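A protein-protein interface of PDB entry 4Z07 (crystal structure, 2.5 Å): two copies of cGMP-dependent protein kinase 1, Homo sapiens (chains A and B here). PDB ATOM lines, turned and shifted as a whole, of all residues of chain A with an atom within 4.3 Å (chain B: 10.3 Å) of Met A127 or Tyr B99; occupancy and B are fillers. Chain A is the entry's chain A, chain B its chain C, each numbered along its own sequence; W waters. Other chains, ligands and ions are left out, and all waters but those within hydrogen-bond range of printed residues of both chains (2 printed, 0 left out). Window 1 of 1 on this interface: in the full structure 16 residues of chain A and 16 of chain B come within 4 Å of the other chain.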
ATOM      1  N   LEU A  33     -20.099  10.939  38.369  1.00  0.00           N
ATOM      2  CA  LEU A  33     -20.354   9.728  37.607  1.00  0.00           C
ATOM      3  C   LEU A  33     -20.599   8.591  38.590  1.00  0.00           C
ATOM      4  O   LEU A  33     -20.103   8.624  39.716  1.00  0.00           O
ATOM      5  CB  LEU A  33     -19.172   9.403  36.698  1.00  0.00           C
ATOM      6  CG  LEU A  33     -18.968  10.312  35.494  1.00  0.00           C
ATOM      7  CD1 LEU A  33     -17.628  10.026  34.858  1.00  0.00           C
ATOM      8  CD2 LEU A  33     -20.100  10.095  34.498  1.00  0.00           C
ATOM      9  N   GLN A  37     -19.320   3.432  36.389  1.00  0.00           N
ATOM     10  CA  GLN A  37     -18.866   4.140  35.194  1.00  0.00           C
ATOM     11  C   GLN A  37     -17.399   4.554  35.262  1.00  0.00           C
ATOM     12  O   GLN A  37     -16.659   4.438  34.292  1.00  0.00           O
ATOM     13  CB  GLN A  37     -19.725   5.380  34.965  1.00  0.00           C
ATOM     14  CG  GLN A  37     -21.165   5.108  34.582  1.00  0.00           C
ATOM     15  CD  GLN A  37     -21.982   6.395  34.546  1.00  0.00           C
ATOM     16  OE1 GLN A  37     -22.098   7.100  35.562  1.00  0.00           O
ATOM     17  NE2 GLN A  37     -22.529   6.726  33.370  1.00  0.00           N
ATOM     18  N   PHE A 123     -16.338   6.382  25.714  1.00  0.00           N
ATOM     19  CA  PHE A 123     -16.888   7.389  26.613  1.00  0.00           C
ATOM     20  C   PHE A 123     -18.403   7.492  26.435  1.00  0.00           C
ATOM     21  O   PHE A 123     -19.148   7.574  27.409  1.00  0.00           O
ATOM     22  CB  PHE A 123     -16.229   8.748  26.388  1.00  0.00           C
ATOM     23  CG  PHE A 123     -16.456   9.716  27.508  1.00  0.00           C
ATOM     24  CD1 PHE A 123     -17.569  10.541  27.526  1.00  0.00           C
ATOM     25  CD2 PHE A 123     -15.557   9.804  28.552  1.00  0.00           C
ATOM     26  CE1 PHE A 123     -17.774  11.442  28.574  1.00  0.00           C
ATOM     27  CE2 PHE A 123     -15.759  10.699  29.604  1.00  0.00           C
ATOM     28  CZ  PHE A 123     -16.869  11.512  29.613  1.00  0.00           C
ATOM     29  N   GLN A 124     -18.848   7.483  25.184  1.00  0.00           N
ATOM     30  CA  GLN A 124     -20.268   7.592  24.867  1.00  0.00           C
ATOM     31  C   GLN A 124     -21.007   6.367  25.384  1.00  0.00           C
ATOM     32  O   GLN A 124     -22.117   6.463  25.915  1.00  0.00           O
ATOM     33  CB  GLN A 124     -20.465   7.733  23.354  1.00  0.00           C
ATOM     34  CG  GLN A 124     -21.918   7.871  22.877  1.00  0.00           C
ATOM     35  CD  GLN A 124     -22.651   6.539  22.707  1.00  0.00           C
ATOM     36  OE1 GLN A 124     -22.040   5.489  22.443  1.00  0.00           O
ATOM     37  NE2 GLN A 124     -23.971   6.582  22.856  1.00  0.00           N
ATOM     38  N   THR A 125     -20.384   5.206  25.223  1.00  0.00           N
ATOM     39  CA  THR A 125     -20.960   3.976  25.736  1.00  0.00           C
ATOM     40  C   THR A 125     -21.095   4.027  27.248  1.00  0.00           C
ATOM     41  O   THR A 125     -22.157   3.747  27.792  1.00  0.00           O
ATOM     42  CB  THR A 125     -20.128   2.754  25.334  1.00  0.00           C
ATOM     43  OG1 THR A 125     -20.199   2.595  23.910  1.00  0.00           O
ATOM     44  CG2 THR A 125     -20.683   1.494  25.999  1.00  0.00           C
ATOM     45  N   ILE A 126     -20.026   4.417  27.925  1.00  0.00           N
ATOM     46  CA  ILE A 126     -20.037   4.430  29.373  1.00  0.00           C
ATOM     47  C   ILE A 126     -21.022   5.464  29.939  1.00  0.00           C
ATOM     48  O   ILE A 126     -21.669   5.210  30.957  1.00  0.00           O
ATOM     49  CB  ILE A 126     -18.622   4.651  29.912  1.00  0.00           C
ATOM     50  CG1 ILE A 126     -17.762   3.429  29.553  1.00  0.00           C
ATOM     51  CG2 ILE A 126     -18.655   4.890  31.419  1.00  0.00           C
ATOM     52  CD1 ILE A 126     -16.261   3.587  29.790  1.00  0.00           C
ATOM     53  N   MET A 127     -21.168   6.603  29.269  1.00  0.00           N
ATOM     54  CA  MET A 127     -22.079   7.659  29.727  1.00  0.00           C
ATOM     55  C   MET A 127     -23.527   7.181  29.807  1.00  0.00           C
ATOM     56  O   MET A 127     -24.352   7.720  30.546  1.00  0.00           O
ATOM     57  CB  MET A 127     -21.998   8.877  28.798  1.00  0.00           C
ATOM     58  CG  MET A 127     -20.730   9.695  28.970  1.00  0.00           C
ATOM     59  SD  MET A 127     -20.383  10.144  30.680  1.00  0.00           S
ATOM     60  CE  MET A 127     -19.088   9.015  31.131  1.00  0.00           C
ATOM     61  N   MET A 128     -23.827   6.162  29.022  1.00  0.00           N
ATOM     62  CA  MET A 128     -25.165   5.619  28.959  1.00  0.00           C
ATOM     63  C   MET A 128     -25.320   4.392  29.864  1.00  0.00           C
ATOM     64  O   MET A 128     -26.415   3.845  29.993  1.00  0.00           O
ATOM     65  CB  MET A 128     -25.502   5.278  27.509  1.00  0.00           C
ATOM     66  CG  MET A 128     -26.980   5.146  27.221  1.00  0.00           C
ATOM     67  SD  MET A 128     -27.263   4.905  25.456  1.00  0.00           S
ATOM     68  CE  MET A 128     -29.029   4.615  25.527  1.00  0.00           C
ATOM     69  N   ARG A 129     -24.226   3.932  30.469  1.00  0.00           N
ATOM     70  CA  ARG A 129     -24.334   2.798  31.386  1.00  0.00           C
ATOM     71  C   ARG A 129     -24.609   3.210  32.828  1.00  0.00           C
ATOM     72  O   ARG A 129     -23.749   3.090  33.700  1.00  0.00           O
ATOM     73  CB  ARG A 129     -23.098   1.913  31.346  1.00  0.00           C
ATOM     74  CG  ARG A 129     -23.069   1.054  30.121  1.00  0.00           C
ATOM     75  CD  ARG A 129     -21.747   0.349  29.935  1.00  0.00           C
ATOM     76  NE  ARG A 129     -21.805  -0.407  28.695  1.00  0.00           N
ATOM     77  CZ  ARG A 129     -20.851  -1.216  28.264  1.00  0.00           C
ATOM     78  NH1 ARG A 129     -19.760  -1.397  28.994  1.00  0.00           N
ATOM     79  NH2 ARG A 129     -20.999  -1.845  27.103  1.00  0.00           N
ATOM     80  N   THR A 130     -25.832   3.666  33.066  1.00  0.00           N
ATOM     81  CA  THR A 130     -26.269   4.077  34.391  1.00  0.00           C
ATOM     82  C   THR A 130     -27.169   3.018  34.995  1.00  0.00           C
ATOM     83  O   THR A 130     -27.665   2.144  34.279  1.00  0.00           O
ATOM     84  CB  THR A 130     -27.053   5.379  34.342  1.00  0.00           C
ATOM     85  OG1 THR A 130     -28.290   5.152  33.651  1.00  0.00           O
ATOM     86  CG2 THR A 130     -26.256   6.443  33.634  1.00  0.00           C
ATOM     87  N   ILE A 133     -30.547   3.362  33.401  1.00  0.00           N
ATOM     88  CA  ILE A 133     -30.641   2.868  32.040  1.00  0.00           C
ATOM     89  C   ILE A 133     -30.693   1.350  32.125  1.00  0.00           C
ATOM     90  O   ILE A 133     -31.518   0.703  31.471  1.00  0.00           O
ATOM     91  CB  ILE A 133     -29.454   3.332  31.157  1.00  0.00           C
ATOM     92  CG1 ILE A 133     -29.578   4.812  30.795  1.00  0.00           C
ATOM     93  CG2 ILE A 133     -29.380   2.511  29.888  1.00  0.00           C
ATOM     94  CD1 ILE A 133     -30.485   5.077  29.625  1.00  0.00           C
ATOM     95  N   ASN B  27     -39.135  13.867  35.163  1.00  0.00           N
ATOM     96  CA  ASN B  27     -38.394  12.942  34.310  1.00  0.00           C
ATOM     97  C   ASN B  27     -37.098  12.513  34.989  1.00  0.00           C
ATOM     98  O   ASN B  27     -36.280  13.350  35.366  1.00  0.00           O
ATOM     99  CB  ASN B  27     -38.118  13.583  32.949  1.00  0.00           C
ATOM    100  CG  ASN B  27     -37.281  12.703  32.039  1.00  0.00           C
ATOM    101  OD1 ASN B  27     -36.054  12.753  32.070  1.00  0.00           O
ATOM    102  ND2 ASN B  27     -37.946  11.909  31.206  1.00  0.00           N
ATOM    103  N   ASP B  28     -36.898  11.208  35.145  1.00  0.00           N
ATOM    104  CA  ASP B  28     -35.759  10.739  35.931  1.00  0.00           C
ATOM    105  C   ASP B  28     -34.400  11.094  35.296  1.00  0.00           C
ATOM    106  O   ASP B  28     -33.403  11.213  36.005  1.00  0.00           O
ATOM    107  CB  ASP B  28     -35.856   9.222  36.157  1.00  0.00           C
ATOM    108  CG  ASP B  28     -36.973   8.835  37.133  1.00  0.00           C
ATOM    109  OD1 ASP B  28     -37.364   9.671  37.980  1.00  0.00           O
ATOM    110  OD2 ASP B  28     -37.462   7.685  37.051  1.00  0.00           O
ATOM    111  N   PHE B  29     -34.365  11.321  33.987  1.00  0.00           N
ATOM    112  CA  PHE B  29     -33.100  11.621  33.311  1.00  0.00           C
ATOM    113  C   PHE B  29     -32.746  13.103  33.237  1.00  0.00           C
ATOM    114  O   PHE B  29     -31.650  13.455  32.810  1.00  0.00           O
ATOM    115  CB  PHE B  29     -33.117  11.066  31.893  1.00  0.00           C
ATOM    116  CG  PHE B  29     -33.467   9.618  31.817  1.00  0.00           C
ATOM    117  CD1 PHE B  29     -34.791   9.214  31.692  1.00  0.00           C
ATOM    118  CD2 PHE B  29     -32.471   8.654  31.867  1.00  0.00           C
ATOM    119  CE1 PHE B  29     -35.117   7.866  31.627  1.00  0.00           C
ATOM    120  CE2 PHE B  29     -32.786   7.306  31.793  1.00  0.00           C
ATOM    121  CZ  PHE B  29     -34.109   6.910  31.679  1.00  0.00           C
ATOM    122  N   MET B  30     -33.661  13.958  33.676  1.00  0.00           N
ATOM    123  CA  MET B  30     -33.510  15.405  33.528  1.00  0.00           C
ATOM    124  C   MET B  30     -33.888  16.190  34.781  1.00  0.00           C
ATOM    125  O   MET B  30     -33.630  17.392  34.864  1.00  0.00           O
ATOM    126  CB  MET B  30     -34.359  15.930  32.373  1.00  0.00           C
ATOM    127  CG  MET B  30     -33.759  15.804  31.023  1.00  0.00           C
ATOM    128  SD  MET B  30     -34.883  16.635  29.897  1.00  0.00           S
ATOM    129  CE  MET B  30     -36.238  15.534  30.129  1.00  0.00           C
ATOM    130  N   LYS B  31     -34.515  15.521  35.743  1.00  0.00           N
ATOM    131  CA  LYS B  31     -35.041  16.200  36.925  1.00  0.00           C
ATOM    132  C   LYS B  31     -33.973  16.938  37.729  1.00  0.00           C
ATOM    133  O   LYS B  31     -34.300  17.821  38.530  1.00  0.00           O
ATOM    134  CB  LYS B  31     -35.751  15.194  37.840  1.00  0.00           C
ATOM    135  CG  LYS B  31     -34.925  13.949  38.163  1.00  0.00           C
ATOM    136  CD  LYS B  31     -35.554  13.090  39.268  1.00  0.00           C
ATOM    137  CE  LYS B  31     -36.994  12.709  38.971  1.00  0.00           C
ATOM    138  NZ  LYS B  31     -37.622  11.980  40.118  1.00  0.00           N
ATOM    139  N   ASN B  32     -32.706  16.599  37.486  1.00  0.00           N
ATOM    140  CA  ASN B  32     -31.589  17.181  38.225  1.00  0.00           C
ATOM    141  C   ASN B  32     -30.834  18.267  37.474  1.00  0.00           C
ATOM    142  O   ASN B  32     -29.707  18.613  37.824  1.00  0.00           O
ATOM    143  CB  ASN B  32     -30.627  16.077  38.637  1.00  0.00           C
ATOM    144  CG  ASN B  32     -31.300  15.029  39.497  1.00  0.00           C
ATOM    145  OD1 ASN B  32     -31.301  13.839  39.167  1.00  0.00           O
ATOM    146  ND2 ASN B  32     -31.897  15.471  40.607  1.00  0.00           N
ATOM    147  N   GLY B  63     -32.093  11.237  16.485  1.00  0.00           N
ATOM    148  CA  GLY B  63     -32.934  12.052  17.328  1.00  0.00           C
ATOM    149  C   GLY B  63     -32.466  13.469  17.164  1.00  0.00           C
ATOM    150  O   GLY B  63     -31.262  13.711  17.058  1.00  0.00           O
ATOM    151  N   VAL B  66     -36.513  17.040  21.471  1.00  0.00           N
ATOM    152  CA  VAL B  66     -36.990  16.551  22.749  1.00  0.00           C
ATOM    153  C   VAL B  66     -38.376  17.123  22.936  1.00  0.00           C
ATOM    154  O   VAL B  66     -38.580  18.313  22.691  1.00  0.00           O
ATOM    155  CB  VAL B  66     -36.081  16.976  23.920  1.00  0.00           C
ATOM    156  CG1 VAL B  66     -36.551  16.333  25.199  1.00  0.00           C
ATOM    157  CG2 VAL B  66     -34.660  16.569  23.657  1.00  0.00           C
ATOM    158  N   GLY B  93     -38.371  11.428  24.121  1.00  0.00           N
ATOM    159  CA  GLY B  93     -37.427  11.753  23.068  1.00  0.00           C
ATOM    160  C   GLY B  93     -36.155  12.404  23.588  1.00  0.00           C
ATOM    161  O   GLY B  93     -35.392  13.000  22.816  1.00  0.00           O
ATOM    162  N   GLU B  94     -35.914  12.305  24.895  1.00  0.00           N
ATOM    163  CA  GLU B  94     -34.723  12.907  25.481  1.00  0.00           C
ATOM    164  C   GLU B  94     -33.511  11.962  25.456  1.00  0.00           C
ATOM    165  O   GLU B  94     -32.369  12.405  25.529  1.00  0.00           O
ATOM    166  CB  GLU B  94     -35.014  13.379  26.917  1.00  0.00           C
ATOM    167  CG  GLU B  94     -34.953  12.277  27.998  1.00  0.00           C
ATOM    168  CD  GLU B  94     -36.174  11.343  27.978  1.00  0.00           C
ATOM    169  OE1 GLU B  94     -36.871  11.250  26.939  1.00  0.00           O
ATOM    170  OE2 GLU B  94     -36.432  10.684  29.008  1.00  0.00           O
ATOM    171  N   LEU B  95     -33.752  10.664  25.351  1.00  0.00           N
ATOM    172  CA  LEU B  95     -32.660   9.713  25.470  1.00  0.00           C
ATOM    173  C   LEU B  95     -31.656   9.887  24.343  1.00  0.00           C
ATOM    174  O   LEU B  95     -30.445   9.975  24.592  1.00  0.00           O
ATOM    175  CB  LEU B  95     -33.190   8.277  25.516  1.00  0.00           C
ATOM    176  CG  LEU B  95     -34.036   7.986  26.765  1.00  0.00           C
ATOM    177  CD1 LEU B  95     -34.544   6.560  26.766  1.00  0.00           C
ATOM    178  CD2 LEU B  95     -33.260   8.258  28.042  1.00  0.00           C
ATOM    179  N   ALA B  96     -32.152   9.987  23.114  1.00  0.00           N
ATOM    180  CA  ALA B  96     -31.268  10.136  21.956  1.00  0.00           C
ATOM    181  C   ALA B  96     -30.400  11.390  22.084  1.00  0.00           C
ATOM    182  O   ALA B  96     -29.268  11.420  21.626  1.00  0.00           O
ATOM    183  CB  ALA B  96     -32.076  10.175  20.662  1.00  0.00           C
ATOM    184  N   ILE B  97     -30.934  12.420  22.724  1.00  0.00           N
ATOM    185  CA  ILE B  97     -30.224  13.688  22.839  1.00  0.00           C
ATOM    186  C   ILE B  97     -29.264  13.702  24.022  1.00  0.00           C
ATOM    187  O   ILE B  97     -28.159  14.232  23.935  1.00  0.00           O
ATOM    188  CB  ILE B  97     -31.209  14.866  22.981  1.00  0.00           C
ATOM    189  CG1 ILE B  97     -32.354  14.739  21.958  1.00  0.00           C
ATOM    190  CG2 ILE B  97     -30.480  16.181  22.894  1.00  0.00           C
ATOM    191  CD1 ILE B  97     -31.933  14.686  20.526  1.00  0.00           C
ATOM    192  N   LEU B  98     -29.710  13.145  25.139  1.00  0.00           N
ATOM    193  CA  LEU B  98     -28.888  13.075  26.328  1.00  0.00           C
ATOM    194  C   LEU B  98     -27.706  12.156  26.144  1.00  0.00           C
ATOM    195  O   LEU B  98     -26.627  12.412  26.670  1.00  0.00           O
ATOM    196  CB  LEU B  98     -29.708  12.597  27.522  1.00  0.00           C
ATOM    197  CG  LEU B  98     -30.589  13.621  28.222  1.00  0.00           C
ATOM    198  CD1 LEU B  98     -31.440  12.905  29.255  1.00  0.00           C
ATOM    199  CD2 LEU B  98     -29.720  14.698  28.884  1.00  0.00           C
ATOM    200  N   TYR B  99     -27.915  11.083  25.395  1.00  0.00           N
ATOM    201  CA  TYR B  99     -26.952   9.997  25.386  1.00  0.00           C
ATOM    202  C   TYR B  99     -26.323   9.784  24.016  1.00  0.00           C
ATOM    203  O   TYR B  99     -25.594   8.813  23.791  1.00  0.00           O
ATOM    204  CB  TYR B  99     -27.630   8.724  25.899  1.00  0.00           C
ATOM    205  CG  TYR B  99     -27.950   8.850  27.356  1.00  0.00           C
ATOM    206  CD1 TYR B  99     -26.932   9.072  28.277  1.00  0.00           C
ATOM    207  CD2 TYR B  99     -29.256   8.786  27.822  1.00  0.00           C
ATOM    208  CE1 TYR B  99     -27.196   9.208  29.624  1.00  0.00           C
ATOM    209  CE2 TYR B  99     -29.538   8.913  29.177  1.00  0.00           C
ATOM    210  CZ  TYR B  99     -28.497   9.126  30.073  1.00  0.00           C
ATOM    211  OH  TYR B  99     -28.734   9.264  31.422  1.00  0.00           O
ATOM    212  N   ASN B 100     -26.604  10.711  23.112  1.00  0.00           N
ATOM    213  CA  ASN B 100     -26.046  10.696  21.763  1.00  0.00           C
ATOM    214  C   ASN B 100     -26.091   9.350  21.073  1.00  0.00           C
ATOM    215  O   ASN B 100     -25.077   8.860  20.608  1.00  0.00           O
ATOM    216  CB  ASN B 100     -24.608  11.203  21.799  1.00  0.00           C
ATOM    217  CG  ASN B 100     -24.535  12.648  22.239  1.00  0.00           C
ATOM    218  OD1 ASN B 100     -24.881  13.562  21.481  1.00  0.00           O
ATOM    219  ND2 ASN B 100     -24.118  12.867  23.478  1.00  0.00           N
ATOM    220  N   CYS B 101     -27.291   8.784  21.016  1.00  0.00           N
ATOM    221  CA  CYS B 101     -27.573   7.526  20.343  1.00  0.00           C
ATOM    222  C   CYS B 101     -28.768   7.691  19.429  1.00  0.00           C
ATOM    223  O   CYS B 101     -29.389   8.749  19.415  1.00  0.00           O
ATOM    224  CB  CYS B 101     -27.849   6.441  21.368  1.00  0.00           C
ATOM    225  SG  CYS B 101     -29.246   6.812  22.507  1.00  0.00           S
ATOM    226  N   THR B 102     -29.090   6.661  18.655  1.00  0.00           N
ATOM    227  CA  THR B 102     -30.314   6.699  17.864  1.00  0.00           C
ATOM    228  C   THR B 102     -31.508   6.500  18.787  1.00  0.00           C
ATOM    229  O   THR B 102     -31.362   6.038  19.925  1.00  0.00           O
ATOM    230  CB  THR B 102     -30.354   5.617  16.748  1.00  0.00           C
ATOM    231  OG1 THR B 102     -30.173   4.322  17.331  1.00  0.00           O
ATOM    232  CG2 THR B 102     -29.275   5.849  15.700  1.00  0.00           C
ATOM    233  N   ARG B 103     -32.687   6.847  18.281  1.00  0.00           N
ATOM    234  CA  ARG B 103     -33.927   6.680  19.025  1.00  0.00           C
ATOM    235  C   ARG B 103     -34.067   5.233  19.498  1.00  0.00           C
ATOM    236  O   ARG B 103     -33.909   4.303  18.718  1.00  0.00           O
ATOM    237  CB  ARG B 103     -35.122   7.095  18.163  1.00  0.00           C
ATOM    238  CG  ARG B 103     -35.105   8.560  17.696  1.00  0.00           C
ATOM    239  CD  ARG B 103     -35.357   9.526  18.851  1.00  0.00           C
ATOM    240  NE  ARG B 103     -35.796  10.826  18.351  1.00  0.00           N
ATOM    241  CZ  ARG B 103     -35.955  11.917  19.098  1.00  0.00           C
ATOM    242  NH1 ARG B 103     -35.708  11.890  20.402  1.00  0.00           N
ATOM    243  NH2 ARG B 103     -36.369  13.041  18.531  1.00  0.00           N
ATOM    244  N   THR B 104     -34.341   5.058  20.788  1.00  0.00           N
ATOM    245  CA  THR B 104     -34.319   3.740  21.409  1.00  0.00           C
ATOM    246  C   THR B 104     -35.670   3.052  21.397  1.00  0.00           C
ATOM    247  O   THR B 104     -35.801   1.917  21.873  1.00  0.00           O
ATOM    248  CB  THR B 104     -33.860   3.829  22.853  1.00  0.00           C
ATOM    249  OG1 THR B 104     -34.864   4.514  23.616  1.00  0.00           O
ATOM    250  CG2 THR B 104     -32.527   4.572  22.931  1.00  0.00           C
ATOM    251  N   ARG B 120     -31.876  19.646  19.188  1.00  0.00           N
ATOM    252  CA  ARG B 120     -30.681  19.142  19.844  1.00  0.00           C
ATOM    253  C   ARG B 120     -29.662  20.208  20.149  1.00  0.00           C
ATOM    254  O   ARG B 120     -29.118  20.265  21.257  1.00  0.00           O
ATOM    255  CB  ARG B 120     -30.020  18.107  18.925  1.00  0.00           C
ATOM    256  CG  ARG B 120     -28.742  17.532  19.425  1.00  0.00           C
ATOM    257  CD  ARG B 120     -28.155  16.583  18.404  1.00  0.00           C
ATOM    258  NE  ARG B 120     -28.867  15.305  18.325  1.00  0.00           N
ATOM    259  CZ  ARG B 120     -28.649  14.270  19.139  1.00  0.00           C
ATOM    260  NH1 ARG B 120     -27.748  14.359  20.112  1.00  0.00           N
ATOM    261  NH2 ARG B 120     -29.339  13.143  18.992  1.00  0.00           N
ATOM    262  N   PHE B 123     -30.747  22.367  23.063  1.00  0.00           N
ATOM    263  CA  PHE B 123     -30.624  21.564  24.256  1.00  0.00           C
ATOM    264  C   PHE B 123     -29.173  21.464  24.704  1.00  0.00           C
ATOM    265  O   PHE B 123     -28.861  21.673  25.873  1.00  0.00           O
ATOM    266  CB  PHE B 123     -31.202  20.168  24.007  1.00  0.00           C
ATOM    267  CG  PHE B 123     -31.368  19.348  25.254  1.00  0.00           C
ATOM    268  CD1 PHE B 123     -30.334  18.540  25.706  1.00  0.00           C
ATOM    269  CD2 PHE B 123     -32.543  19.394  25.981  1.00  0.00           C
ATOM    270  CE1 PHE B 123     -30.467  17.790  26.849  1.00  0.00           C
ATOM    271  CE2 PHE B 123     -32.685  18.645  27.127  1.00  0.00           C
ATOM    272  CZ  PHE B 123     -31.650  17.841  27.562  1.00  0.00           C
ATOM    273  N   GLN B 124     -28.281  21.187  23.764  1.00  0.00           N
ATOM    274  CA  GLN B 124     -26.872  21.027  24.107  1.00  0.00           C
ATOM    275  C   GLN B 124     -26.261  22.347  24.568  1.00  0.00           C
ATOM    276  O   GLN B 124     -25.443  22.367  25.493  1.00  0.00           O
ATOM    277  CB  GLN B 124     -26.101  20.421  22.928  1.00  0.00           C
ATOM    278  CG  GLN B 124     -26.382  18.917  22.819  1.00  0.00           C
ATOM    279  CD  GLN B 124     -25.669  18.238  21.667  1.00  0.00           C
ATOM    280  OE1 GLN B 124     -25.220  18.890  20.716  1.00  0.00           O
ATOM    281  NE2 GLN B 124     -25.565  16.911  21.745  1.00  0.00           N
ATOM    282  N   MET B 127     -27.351  22.777  28.075  1.00  0.00           N
ATOM    283  CA  MET B 127     -26.707  21.803  28.969  1.00  0.00           C
ATOM    284  C   MET B 127     -25.382  22.313  29.496  1.00  0.00           C
ATOM    285  O   MET B 127     -24.920  21.893  30.554  1.00  0.00           O
ATOM    286  CB  MET B 127     -26.481  20.471  28.256  1.00  0.00           C
ATOM    287  CG  MET B 127     -27.727  19.626  28.069  1.00  0.00           C
ATOM    288  SD  MET B 127     -28.636  19.405  29.612  1.00  0.00           S
ATOM    289  CE  MET B 127     -30.030  20.496  29.364  1.00  0.00           C
HETATM  290  O   HOH W   1     -29.469   7.512  33.245  1.00  0.00           O
HETATM  291  O   HOH W   2     -23.974   8.146  25.846  1.00  0.00           O
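The side-chain amide nitrogen (NE2) of Gln A124 is in hydrogen-bond range of the backbone carbonyl oxygen (O) of Tyr B99 (2.9 Å). NE2 of Gln A124 lies within hydrogen-bond range of O of Asn B100 (3.4 Å).
The side-chain hydroxyl (OG1) of Thr A130 lies within hydrogen-bond range of the backbone NH (N) of Ile A133, at 2.9 Å. The side-chain amide oxygen of Asn B27 is in hydrogen-bond range of the backbone NH of Phe B29, at 2.9 Å. O of Ala B96 sits at hydrogen-bond distance from N of Cys B101, 3.4 Å away. OD1 of Asn B100 is in hydrogen-bond range of NH1 of Arg B120, 3.3 Å away. The side-chain amide oxygen (OD1) of Asn B100 sits at hydrogen-bond distance from the side-chain amide nitrogen (NE2) of Gln B124 (3.4 Å).
Among the printed residues, pairs that only touch across the chains: Met A127 with Tyr B99 (3.3 Å), Met A128 with Cys B101 (3.7 Å), Met A128 with Tyr B99 (3.8 Å), Ile A133 with Phe B29 (3.9 Å) and Ile A133 with Tyr B99 (3.98 Å).
Met A127 touches one residue of chain B. Of the printed residues of chain A, Tyr B99 touches Gln A124 (2.9 Å), Met A127 (3.3 Å), Met A128 (3.8 Å) and Ile A133 (3.98 Å). No residue of chain B comes within 4 Å of Phe A123. Gln A124 touches two residues of chain B. Of the printed residues of chain B, Ile A133 touches Phe B29 (3.9 Å) and Tyr B99 (3.98 Å). Printed residues of chain A within 4 Å of Phe B29: Ile A133 (3.9 Å). Met B127 touches none of the printed residues of chain A. The nearest residue of chain B that does not touch Met A127 is Leu B98 (6.2 Å). The nearest printed residue of chain A that does not touch Tyr B99 is Thr A130 (4.4 Å). The nearest printed residue of chain A that does not touch Cys B101 is Gln A124 (4.2 Å).
Hydrophobic or aromatic side chains of chain A that line the printed part of chain B: Met A128 and Ile A133. Along chain A the printed residues that touch a printed residue of chain B span positions 124 to 133. Of the 24 printed residues of chain B, 4 touch a printed residue of chain A. Hydrophobic or aromatic side chains of chain B within 4 Å of the printed part of chain A: Phe B29 and Tyr B99.
Positions printed for both chains: 123, 124 and 127. Of the 7 pairs that touch across the chains among the printed residues, none has its exchanged pair printed and touching as well.
Water W2 bridges O of Gln A124 (2.5 Å) and O of Tyr B99 (2.7 Å). Water W1 lies within hydrogen-bond range of the side-chain hydroxyl of Tyr B99 and the side-chain hydroxyl of Thr A130.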
